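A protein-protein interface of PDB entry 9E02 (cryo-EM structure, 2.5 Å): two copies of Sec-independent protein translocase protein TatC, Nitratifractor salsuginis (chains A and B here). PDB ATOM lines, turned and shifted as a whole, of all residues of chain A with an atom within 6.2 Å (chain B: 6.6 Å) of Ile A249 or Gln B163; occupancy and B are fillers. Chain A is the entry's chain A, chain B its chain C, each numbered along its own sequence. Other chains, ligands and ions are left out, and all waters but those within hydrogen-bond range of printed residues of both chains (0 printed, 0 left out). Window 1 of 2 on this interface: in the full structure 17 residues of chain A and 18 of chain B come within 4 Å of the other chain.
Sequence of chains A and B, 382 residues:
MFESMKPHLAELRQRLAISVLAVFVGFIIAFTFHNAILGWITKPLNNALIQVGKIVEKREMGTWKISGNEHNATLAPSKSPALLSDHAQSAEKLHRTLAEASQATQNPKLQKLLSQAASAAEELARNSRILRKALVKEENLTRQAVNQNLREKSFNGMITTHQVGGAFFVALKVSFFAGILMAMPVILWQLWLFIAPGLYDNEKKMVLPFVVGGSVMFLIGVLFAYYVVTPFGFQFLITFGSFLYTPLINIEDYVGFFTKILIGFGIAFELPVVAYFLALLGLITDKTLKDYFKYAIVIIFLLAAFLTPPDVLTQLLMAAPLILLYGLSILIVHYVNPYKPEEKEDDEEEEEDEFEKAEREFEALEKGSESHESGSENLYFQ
The backbone carbonyl oxygen of Thr A246 lies within hydrogen-bond range of the backbone NH of Thr B161 (2.9 Å).
The side-chain amide nitrogen (ND2) of Asn A250 lies within hydrogen-bond range of the backbone carbonyl oxygen (O) of His B162 (3.1 Å).
N of Leu A248 lies within hydrogen-bond range of O of Thr B161, at 2.7 Å.
The side-chain amide oxygen (OE1) of Gln B163 lies close to the side-chain carboxylate (OD2) of Asp A253 (3.0 Å).
The backbone NH (N) of Met A158 lies within hydrogen-bond range of the backbone carbonyl oxygen (O) of Pro A247, 3.4 Å away.
The side-chain amide oxygen of Asn A250 lies close to the side-chain carboxylate of Asp A253 (3.3 Å).
NE2 of His B162 is in hydrogen-bond range of ND2 of Asn B250, 2.8 Å away.
ND1 of His B162 lies close to OE1 of Gln B163 (3.3 Å).
N of His B162 lies close to OE2 of Glu B252 (3.3 Å).
N of Ile A249 sits at hydrogen-bond distance from O of Met A158, at 3.4 Å.
Leu A237 touches Val B164 (CB to CB, 3.3 Å).
CD2 of Leu A237 touches CB of Phe B168, at 3.6 Å.
Ile A238 touches Val B164.
Thr B161 touches Pro A247.
Leu A248 touches His B162.
Thr B161 touches Ile A249.
Ile A249 touches His B162.
Ile A249 touches Gln B163 (CD1 to N, 3.4 Å).
His B162 touches Asp A253.
Printed residues of chain B within 4 Å of Thr A246: Thr B161 (2.9 Å).
Ile A249 touches just these residues of chain B: Thr B161, His B162 and Gln B163.
Gln B163 touches just these residues of chain A: Ile A249 and Asp A253.
Of the printed residues of chain A, Val B164 touches Leu A237 (3.3 Å) and Ile A238 (3.3 Å).
Of the printed residues of chain A, Phe B168 touches Leu A237 (3.6 Å).
Glu B252 touches none of the printed residues of chain A.
The nearest residue of chain B that does not touch Ile A249 is Val B164 (4.2 Å).
The nearest residue of chain A that does not touch Gln B163 is Asn A250 (4.5 Å).
Hydrophobic or aromatic side chains of chain B within 4 Å of the printed part of chain A: His B162, Val B164 and Phe B168.
Printed residues of chain A that touch a printed residue of chain B: Leu A237, Ile A238, Thr A246, Pro A247, Leu A248, Ile A249, Asn A250 and Asp A253.
Hydrophobic or aromatic side chains of chain A within 4 Å of the printed part of chain B: Leu A237, Ile A238 and Ile A249.
Among the printed residues, 13 pairs touch across the chains.
Among the printed residues, no Asp or Glu carboxylate lies within 4 Å of a Lys or Arg side-chain nitrogen of the other chain.
2 positions are printed for both chains.
Of the 13 pairs that touch across the chains among the printed residues, none has its exchanged pair printed and touching as well.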
ATOM      1  N   LEU A  45       3.041  31.212 -23.130  1.00  0.00           N
ATOM      2  CA  LEU A  45       1.998  31.140 -24.146  1.00  0.00           C
ATOM      3  C   LEU A  45       2.222  32.182 -25.234  1.00  0.00           C
ATOM      4  O   LEU A  45       2.154  31.874 -26.428  1.00  0.00           O
ATOM      5  CB  LEU A  45       0.629  31.316 -23.494  1.00  0.00           C
ATOM      6  CG  LEU A  45      -0.604  30.981 -24.333  1.00  0.00           C
ATOM      7  CD1 LEU A  45      -0.472  29.607 -24.955  1.00  0.00           C
ATOM      8  CD2 LEU A  45      -1.851  31.063 -23.479  1.00  0.00           C
ATOM      9  N   LEU A  49       3.204  31.408 -29.112  1.00  0.00           N
ATOM     10  CA  LEU A  49       2.339  31.921 -30.165  1.00  0.00           C
ATOM     11  C   LEU A  49       3.125  32.739 -31.177  1.00  0.00           C
ATOM     12  O   LEU A  49       2.921  32.596 -32.386  1.00  0.00           O
ATOM     13  CB  LEU A  49       1.209  32.746 -29.563  1.00  0.00           C
ATOM     14  CG  LEU A  49       0.096  31.919 -28.923  1.00  0.00           C
ATOM     15  CD1 LEU A  49      -0.805  32.794 -28.073  1.00  0.00           C
ATOM     16  CD2 LEU A  49      -0.698  31.172 -29.970  1.00  0.00           C
ATOM     17  N   GLY A 157      -3.481  33.581 -34.074  1.00  0.00           N
ATOM     18  CA  GLY A 157      -3.822  33.143 -32.737  1.00  0.00           C
ATOM     19  C   GLY A 157      -3.221  34.048 -31.680  1.00  0.00           C
ATOM     20  O   GLY A 157      -2.155  34.632 -31.875  1.00  0.00           O
ATOM     21  N   MET A 158      -3.922  34.159 -30.554  1.00  0.00           N
ATOM     22  CA  MET A 158      -3.467  34.918 -29.395  1.00  0.00           C
ATOM     23  C   MET A 158      -4.340  34.520 -28.210  1.00  0.00           C
ATOM     24  O   MET A 158      -5.236  33.683 -28.335  1.00  0.00           O
ATOM     25  CB  MET A 158      -3.504  36.427 -29.663  1.00  0.00           C
ATOM     26  CG  MET A 158      -2.571  37.257 -28.782  1.00  0.00           C
ATOM     27  SD  MET A 158      -1.019  36.440 -28.352  1.00  0.00           S
ATOM     28  CE  MET A 158      -0.049  36.666 -29.842  1.00  0.00           C
ATOM     29  N   ILE A 159      -4.063  35.114 -27.051  1.00  0.00           N
ATOM     30  CA  ILE A 159      -4.790  34.772 -25.833  1.00  0.00           C
ATOM     31  C   ILE A 159      -6.128  35.495 -25.818  1.00  0.00           C
ATOM     32  O   ILE A 159      -6.199  36.708 -26.047  1.00  0.00           O
ATOM     33  CB  ILE A 159      -3.965  35.107 -24.583  1.00  0.00           C
ATOM     34  CG1 ILE A 159      -2.514  34.675 -24.770  1.00  0.00           C
ATOM     35  CG2 ILE A 159      -4.565  34.431 -23.366  1.00  0.00           C
ATOM     36  CD1 ILE A 159      -1.653  34.977 -23.586  1.00  0.00           C
ATOM     37  N   THR A 160      -7.189  34.752 -25.529  1.00  0.00           N
ATOM     38  CA  THR A 160      -8.554  35.244 -25.574  1.00  0.00           C
ATOM     39  C   THR A 160      -9.234  35.019 -24.230  1.00  0.00           C
ATOM     40  O   THR A 160      -8.684  34.400 -23.319  1.00  0.00           O
ATOM     41  CB  THR A 160      -9.353  34.549 -26.687  1.00  0.00           C
ATOM     42  OG1 THR A 160      -9.522  33.165 -26.364  1.00  0.00           O
ATOM     43  CG2 THR A 160      -8.629  34.657 -28.010  1.00  0.00           C
ATOM     44  N   THR A 161     -10.444  35.559 -24.115  1.00  0.00           N
ATOM     45  CA  THR A 161     -11.345  35.279 -23.005  1.00  0.00           C
ATOM     46  C   THR A 161     -12.699  34.912 -23.589  1.00  0.00           C
ATOM     47  O   THR A 161     -13.287  35.699 -24.335  1.00  0.00           O
ATOM     48  CB  THR A 161     -11.486  36.478 -22.064  1.00  0.00           C
ATOM     49  OG1 THR A 161     -10.594  37.522 -22.469  1.00  0.00           O
ATOM     50  CG2 THR A 161     -11.174  36.075 -20.640  1.00  0.00           C
ATOM     51  N   LEU A 237       3.211  21.860 -29.150  1.00  0.00           N
ATOM     52  CA  LEU A 237       1.769  21.655 -29.134  1.00  0.00           C
ATOM     53  C   LEU A 237       1.039  22.670 -30.008  1.00  0.00           C
ATOM     54  O   LEU A 237       0.055  22.321 -30.670  1.00  0.00           O
ATOM     55  CB  LEU A 237       1.262  21.696 -27.699  1.00  0.00           C
ATOM     56  CG  LEU A 237       1.698  20.583 -26.746  1.00  0.00           C
ATOM     57  CD1 LEU A 237       1.244  20.875 -25.333  1.00  0.00           C
ATOM     58  CD2 LEU A 237       1.164  19.243 -27.201  1.00  0.00           C
ATOM     59  N   ILE A 238       1.486  23.930 -30.023  1.00  0.00           N
ATOM     60  CA  ILE A 238       0.907  24.890 -30.960  1.00  0.00           C
ATOM     61  C   ILE A 238       1.214  24.495 -32.399  1.00  0.00           C
ATOM     62  O   ILE A 238       0.335  24.547 -33.267  1.00  0.00           O
ATOM     63  CB  ILE A 238       1.377  26.325 -30.659  1.00  0.00           C
ATOM     64  CG1 ILE A 238       0.882  26.806 -29.304  1.00  0.00           C
ATOM     65  CG2 ILE A 238       0.780  27.276 -31.669  1.00  0.00           C
ATOM     66  CD1 ILE A 238      -0.615  26.752 -29.198  1.00  0.00           C
ATOM     67  N   THR A 246      -6.754  27.344 -35.988  1.00  0.00           N
ATOM     68  CA  THR A 246      -6.249  28.628 -35.536  1.00  0.00           C
ATOM     69  C   THR A 246      -6.256  28.656 -34.019  1.00  0.00           C
ATOM     70  O   THR A 246      -7.318  28.457 -33.413  1.00  0.00           O
ATOM     71  CB  THR A 246      -7.091  29.770 -36.093  1.00  0.00           C
ATOM     72  OG1 THR A 246      -6.847  29.903 -37.496  1.00  0.00           O
ATOM     73  CG2 THR A 246      -6.745  31.072 -35.411  1.00  0.00           C
ATOM     74  N   PRO A 247      -5.118  28.891 -33.368  1.00  0.00           N
ATOM     75  CA  PRO A 247      -5.004  28.792 -31.897  1.00  0.00           C
ATOM     76  C   PRO A 247      -5.597  29.979 -31.141  1.00  0.00           C
ATOM     77  O   PRO A 247      -4.926  30.938 -30.770  1.00  0.00           O
ATOM     78  CB  PRO A 247      -3.490  28.695 -31.683  1.00  0.00           C
ATOM     79  CG  PRO A 247      -2.866  28.629 -33.049  1.00  0.00           C
ATOM     80  CD  PRO A 247      -3.833  29.244 -33.982  1.00  0.00           C
ATOM     81  N   LEU A 248      -6.903  29.924 -30.898  1.00  0.00           N
ATOM     82  CA  LEU A 248      -7.575  30.943 -30.090  1.00  0.00           C
ATOM     83  C   LEU A 248      -7.595  30.493 -28.628  1.00  0.00           C
ATOM     84  O   LEU A 248      -8.630  30.169 -28.047  1.00  0.00           O
ATOM     85  CB  LEU A 248      -8.975  31.209 -30.625  1.00  0.00           C
ATOM     86  CG  LEU A 248      -9.047  31.861 -32.006  1.00  0.00           C
ATOM     87  CD1 LEU A 248     -10.476  32.207 -32.357  1.00  0.00           C
ATOM     88  CD2 LEU A 248      -8.169  33.093 -32.065  1.00  0.00           C
ATOM     89  N   ILE A 249      -6.402  30.494 -28.033  1.00  0.00           N
ATOM     90  CA  ILE A 249      -6.213  29.937 -26.698  1.00  0.00           C
ATOM     91  C   ILE A 249      -6.817  30.870 -25.659  1.00  0.00           C
ATOM     92  O   ILE A 249      -6.452  32.048 -25.569  1.00  0.00           O
ATOM     93  CB  ILE A 249      -4.720  29.698 -26.425  1.00  0.00           C
ATOM     94  CG1 ILE A 249      -4.050  29.048 -27.637  1.00  0.00           C
ATOM     95  CG2 ILE A 249      -4.523  28.856 -25.178  1.00  0.00           C
ATOM     96  CD1 ILE A 249      -4.507  27.642 -27.902  1.00  0.00           C
ATOM     97  N   ASN A 250      -7.736  30.343 -24.861  1.00  0.00           N
ATOM     98  CA  ASN A 250      -8.393  31.127 -23.828  1.00  0.00           C
ATOM     99  C   ASN A 250      -7.719  30.905 -22.480  1.00  0.00           C
ATOM    100  O   ASN A 250      -7.245  29.811 -22.167  1.00  0.00           O
ATOM    101  CB  ASN A 250      -9.886  30.792 -23.758  1.00  0.00           C
ATOM    102  CG  ASN A 250     -10.164  29.448 -23.130  1.00  0.00           C
ATOM    103  OD1 ASN A 250     -10.779  29.361 -22.072  1.00  0.00           O
ATOM    104  ND2 ASN A 250      -9.724  28.386 -23.790  1.00  0.00           N
ATOM    105  N   ILE A 251      -7.675  31.974 -21.687  1.00  0.00           N
ATOM    106  CA  ILE A 251      -6.910  31.976 -20.447  1.00  0.00           C
ATOM    107  C   ILE A 251      -7.531  31.056 -19.401  1.00  0.00           C
ATOM    108  O   ILE A 251      -6.823  30.526 -18.537  1.00  0.00           O
ATOM    109  CB  ILE A 251      -6.772  33.423 -19.936  1.00  0.00           C
ATOM    110  CG1 ILE A 251      -5.772  33.504 -18.783  1.00  0.00           C
ATOM    111  CG2 ILE A 251      -8.126  33.995 -19.527  1.00  0.00           C
ATOM    112  CD1 ILE A 251      -4.437  32.923 -19.111  1.00  0.00           C
ATOM    113  N   ASP A 253      -8.971  27.954 -19.449  1.00  0.00           N
ATOM    114  CA  ASP A 253      -8.441  26.598 -19.433  1.00  0.00           C
ATOM    115  C   ASP A 253      -6.923  26.583 -19.324  1.00  0.00           C
ATOM    116  O   ASP A 253      -6.352  25.653 -18.737  1.00  0.00           O
ATOM    117  CB  ASP A 253      -8.889  25.850 -20.688  1.00  0.00           C
ATOM    118  CG  ASP A 253     -10.393  25.676 -20.755  1.00  0.00           C
ATOM    119  OD1 ASP A 253     -11.116  26.571 -20.271  1.00  0.00           O
ATOM    120  OD2 ASP A 253     -10.851  24.647 -21.292  1.00  0.00           O
ATOM    121  N   TYR A 254      -6.263  27.600 -19.879  1.00  0.00           N
ATOM    122  CA  TYR A 254      -4.809  27.623 -19.895  1.00  0.00           C
ATOM    123  C   TYR A 254      -4.232  27.732 -18.494  1.00  0.00           C
ATOM    124  O   TYR A 254      -3.218  27.099 -18.191  1.00  0.00           O
ATOM    125  CB  TYR A 254      -4.306  28.776 -20.757  1.00  0.00           C
ATOM    126  CG  TYR A 254      -2.834  29.028 -20.584  1.00  0.00           C
ATOM    127  CD1 TYR A 254      -1.899  28.163 -21.126  1.00  0.00           C
ATOM    128  CD2 TYR A 254      -2.376  30.119 -19.863  1.00  0.00           C
ATOM    129  CE1 TYR A 254      -0.554  28.385 -20.967  1.00  0.00           C
ATOM    130  CE2 TYR A 254      -1.032  30.348 -19.699  1.00  0.00           C
ATOM    131  CZ  TYR A 254      -0.125  29.478 -20.252  1.00  0.00           C
ATOM    132  OH  TYR A 254       1.219  29.705 -20.089  1.00  0.00           O
ATOM    133  N   THR B 161      -8.622  26.156 -32.189  1.00  0.00           N
ATOM    134  CA  THR B 161      -8.197  25.431 -30.999  1.00  0.00           C
ATOM    135  C   THR B 161      -8.106  26.430 -29.858  1.00  0.00           C
ATOM    136  O   THR B 161      -7.498  27.494 -30.015  1.00  0.00           O
ATOM    137  CB  THR B 161      -6.846  24.741 -31.204  1.00  0.00           C
ATOM    138  OG1 THR B 161      -6.407  24.920 -32.555  1.00  0.00           O
ATOM    139  CG2 THR B 161      -6.953  23.265 -30.905  1.00  0.00           C
ATOM    140  N   HIS B 162      -8.708  26.101 -28.720  1.00  0.00           N
ATOM    141  CA  HIS B 162      -8.577  26.937 -27.538  1.00  0.00           C
ATOM    142  C   HIS B 162      -7.603  26.353 -26.524  1.00  0.00           C
ATOM    143  O   HIS B 162      -7.553  26.829 -25.388  1.00  0.00           O
ATOM    144  CB  HIS B 162      -9.938  27.175 -26.873  1.00  0.00           C
ATOM    145  CG  HIS B 162     -10.639  25.926 -26.439  1.00  0.00           C
ATOM    146  ND1 HIS B 162     -11.357  25.854 -25.265  1.00  0.00           N
ATOM    147  CD2 HIS B 162     -10.721  24.701 -27.005  1.00  0.00           C
ATOM    148  CE1 HIS B 162     -11.858  24.640 -25.132  1.00  0.00           C
ATOM    149  NE2 HIS B 162     -11.482  23.919 -26.172  1.00  0.00           N
ATOM    150  N   GLN B 163      -6.842  25.325 -26.902  1.00  0.00           N
ATOM    151  CA  GLN B 163      -5.824  24.768 -26.022  1.00  0.00           C
ATOM    152  C   GLN B 163      -4.804  23.976 -26.832  1.00  0.00           C
ATOM    153  O   GLN B 163      -5.100  23.512 -27.935  1.00  0.00           O
ATOM    154  CB  GLN B 163      -6.449  23.891 -24.934  1.00  0.00           C
ATOM    155  CG  GLN B 163      -7.703  23.165 -25.346  1.00  0.00           C
ATOM    156  CD  GLN B 163      -8.649  22.953 -24.188  1.00  0.00           C
ATOM    157  OE1 GLN B 163      -9.189  23.905 -23.631  1.00  0.00           O
ATOM    158  NE2 GLN B 163      -8.859  21.698 -23.815  1.00  0.00           N
ATOM    159  N   VAL B 164      -3.599  23.843 -26.270  1.00  0.00           N
ATOM    160  CA  VAL B 164      -2.531  23.051 -26.885  1.00  0.00           C
ATOM    161  C   VAL B 164      -2.857  21.560 -26.804  1.00  0.00           C
ATOM    162  O   VAL B 164      -2.845  20.820 -27.812  1.00  0.00           O
ATOM    163  CB  VAL B 164      -1.194  23.366 -26.193  1.00  0.00           C
ATOM    164  CG1 VAL B 164      -0.667  24.685 -26.634  1.00  0.00           C
ATOM    165  CG2 VAL B 164      -1.366  23.414 -24.687  1.00  0.00           C
ATOM    166  N   GLY B 165      -3.155  21.104 -25.592  1.00  0.00           N
ATOM    167  CA  GLY B 165      -3.757  19.817 -25.371  1.00  0.00           C
ATOM    168  C   GLY B 165      -4.945  19.668 -26.286  1.00  0.00           C
ATOM    169  O   GLY B 165      -5.283  18.557 -26.658  1.00  0.00           O
ATOM    170  N   GLY B 166      -5.555  20.776 -26.694  1.00  0.00           N
ATOM    171  CA  GLY B 166      -6.603  20.714 -27.683  1.00  0.00           C
ATOM    172  C   GLY B 166      -6.231  19.927 -28.921  1.00  0.00           C
ATOM    173  O   GLY B 166      -6.758  18.837 -29.133  1.00  0.00           O
ATOM    174  N   ALA B 167      -5.309  20.447 -29.730  1.00  0.00           N
ATOM    175  CA  ALA B 167      -4.969  19.775 -30.978  1.00  0.00           C
ATOM    176  C   ALA B 167      -4.316  18.423 -30.719  1.00  0.00           C
ATOM    177  O   ALA B 167      -4.667  17.416 -31.353  1.00  0.00           O
ATOM    178  CB  ALA B 167      -4.058  20.662 -31.824  1.00  0.00           C
ATOM    179  N   PHE B 168      -3.365  18.370 -29.775  1.00  0.00           N
ATOM    180  CA  PHE B 168      -2.666  17.098 -29.589  1.00  0.00           C
ATOM    181  C   PHE B 168      -3.605  16.020 -29.055  1.00  0.00           C
ATOM    182  O   PHE B 168      -3.599  14.876 -29.523  1.00  0.00           O
ATOM    183  CB  PHE B 168      -1.462  17.267 -28.666  1.00  0.00           C
ATOM    184  CG  PHE B 168      -0.522  16.099 -28.701  1.00  0.00           C
ATOM    185  CD1 PHE B 168      -0.027  15.629 -29.902  1.00  0.00           C
ATOM    186  CD2 PHE B 168      -0.160  15.447 -27.537  1.00  0.00           C
ATOM    187  CE1 PHE B 168       0.825  14.550 -29.939  1.00  0.00           C
ATOM    188  CE2 PHE B 168       0.691  14.368 -27.571  1.00  0.00           C
ATOM    189  CZ  PHE B 168       1.184  13.919 -28.775  1.00  0.00           C
ATOM    190  N   ASN B 250     -14.507  25.132 -32.214  1.00  0.00           N
ATOM    191  CA  ASN B 250     -13.295  24.493 -31.732  1.00  0.00           C
ATOM    192  C   ASN B 250     -13.329  22.991 -31.989  1.00  0.00           C
ATOM    193  O   ASN B 250     -14.386  22.358 -31.986  1.00  0.00           O
ATOM    194  CB  ASN B 250     -13.089  24.794 -30.243  1.00  0.00           C
ATOM    195  CG  ASN B 250     -13.956  23.947 -29.339  1.00  0.00           C
ATOM    196  OD1 ASN B 250     -15.064  23.553 -29.700  1.00  0.00           O
ATOM    197  ND2 ASN B 250     -13.454  23.663 -28.152  1.00  0.00           N
ATOM    198  N   GLU B 252     -12.002  20.565 -30.226  1.00  0.00           N
ATOM    199  CA  GLU B 252     -12.072  19.699 -29.053  1.00  0.00           C
ATOM    200  C   GLU B 252     -13.497  19.240 -28.785  1.00  0.00           C
ATOM    201  O   GLU B 252     -13.753  18.044 -28.606  1.00  0.00           O
ATOM    202  CB  GLU B 252     -11.503  20.433 -27.843  1.00  0.00           C
ATOM    203  CG  GLU B 252     -10.043  20.799 -27.993  1.00  0.00           C
ATOM    204  CD  GLU B 252      -9.846  22.163 -28.626  1.00  0.00           C
ATOM    205  OE1 GLU B 252     -10.729  22.602 -29.391  1.00  0.00           O
ATOM    206  OE2 GLU B 252      -8.811  22.802 -28.360  1.00  0.00           O
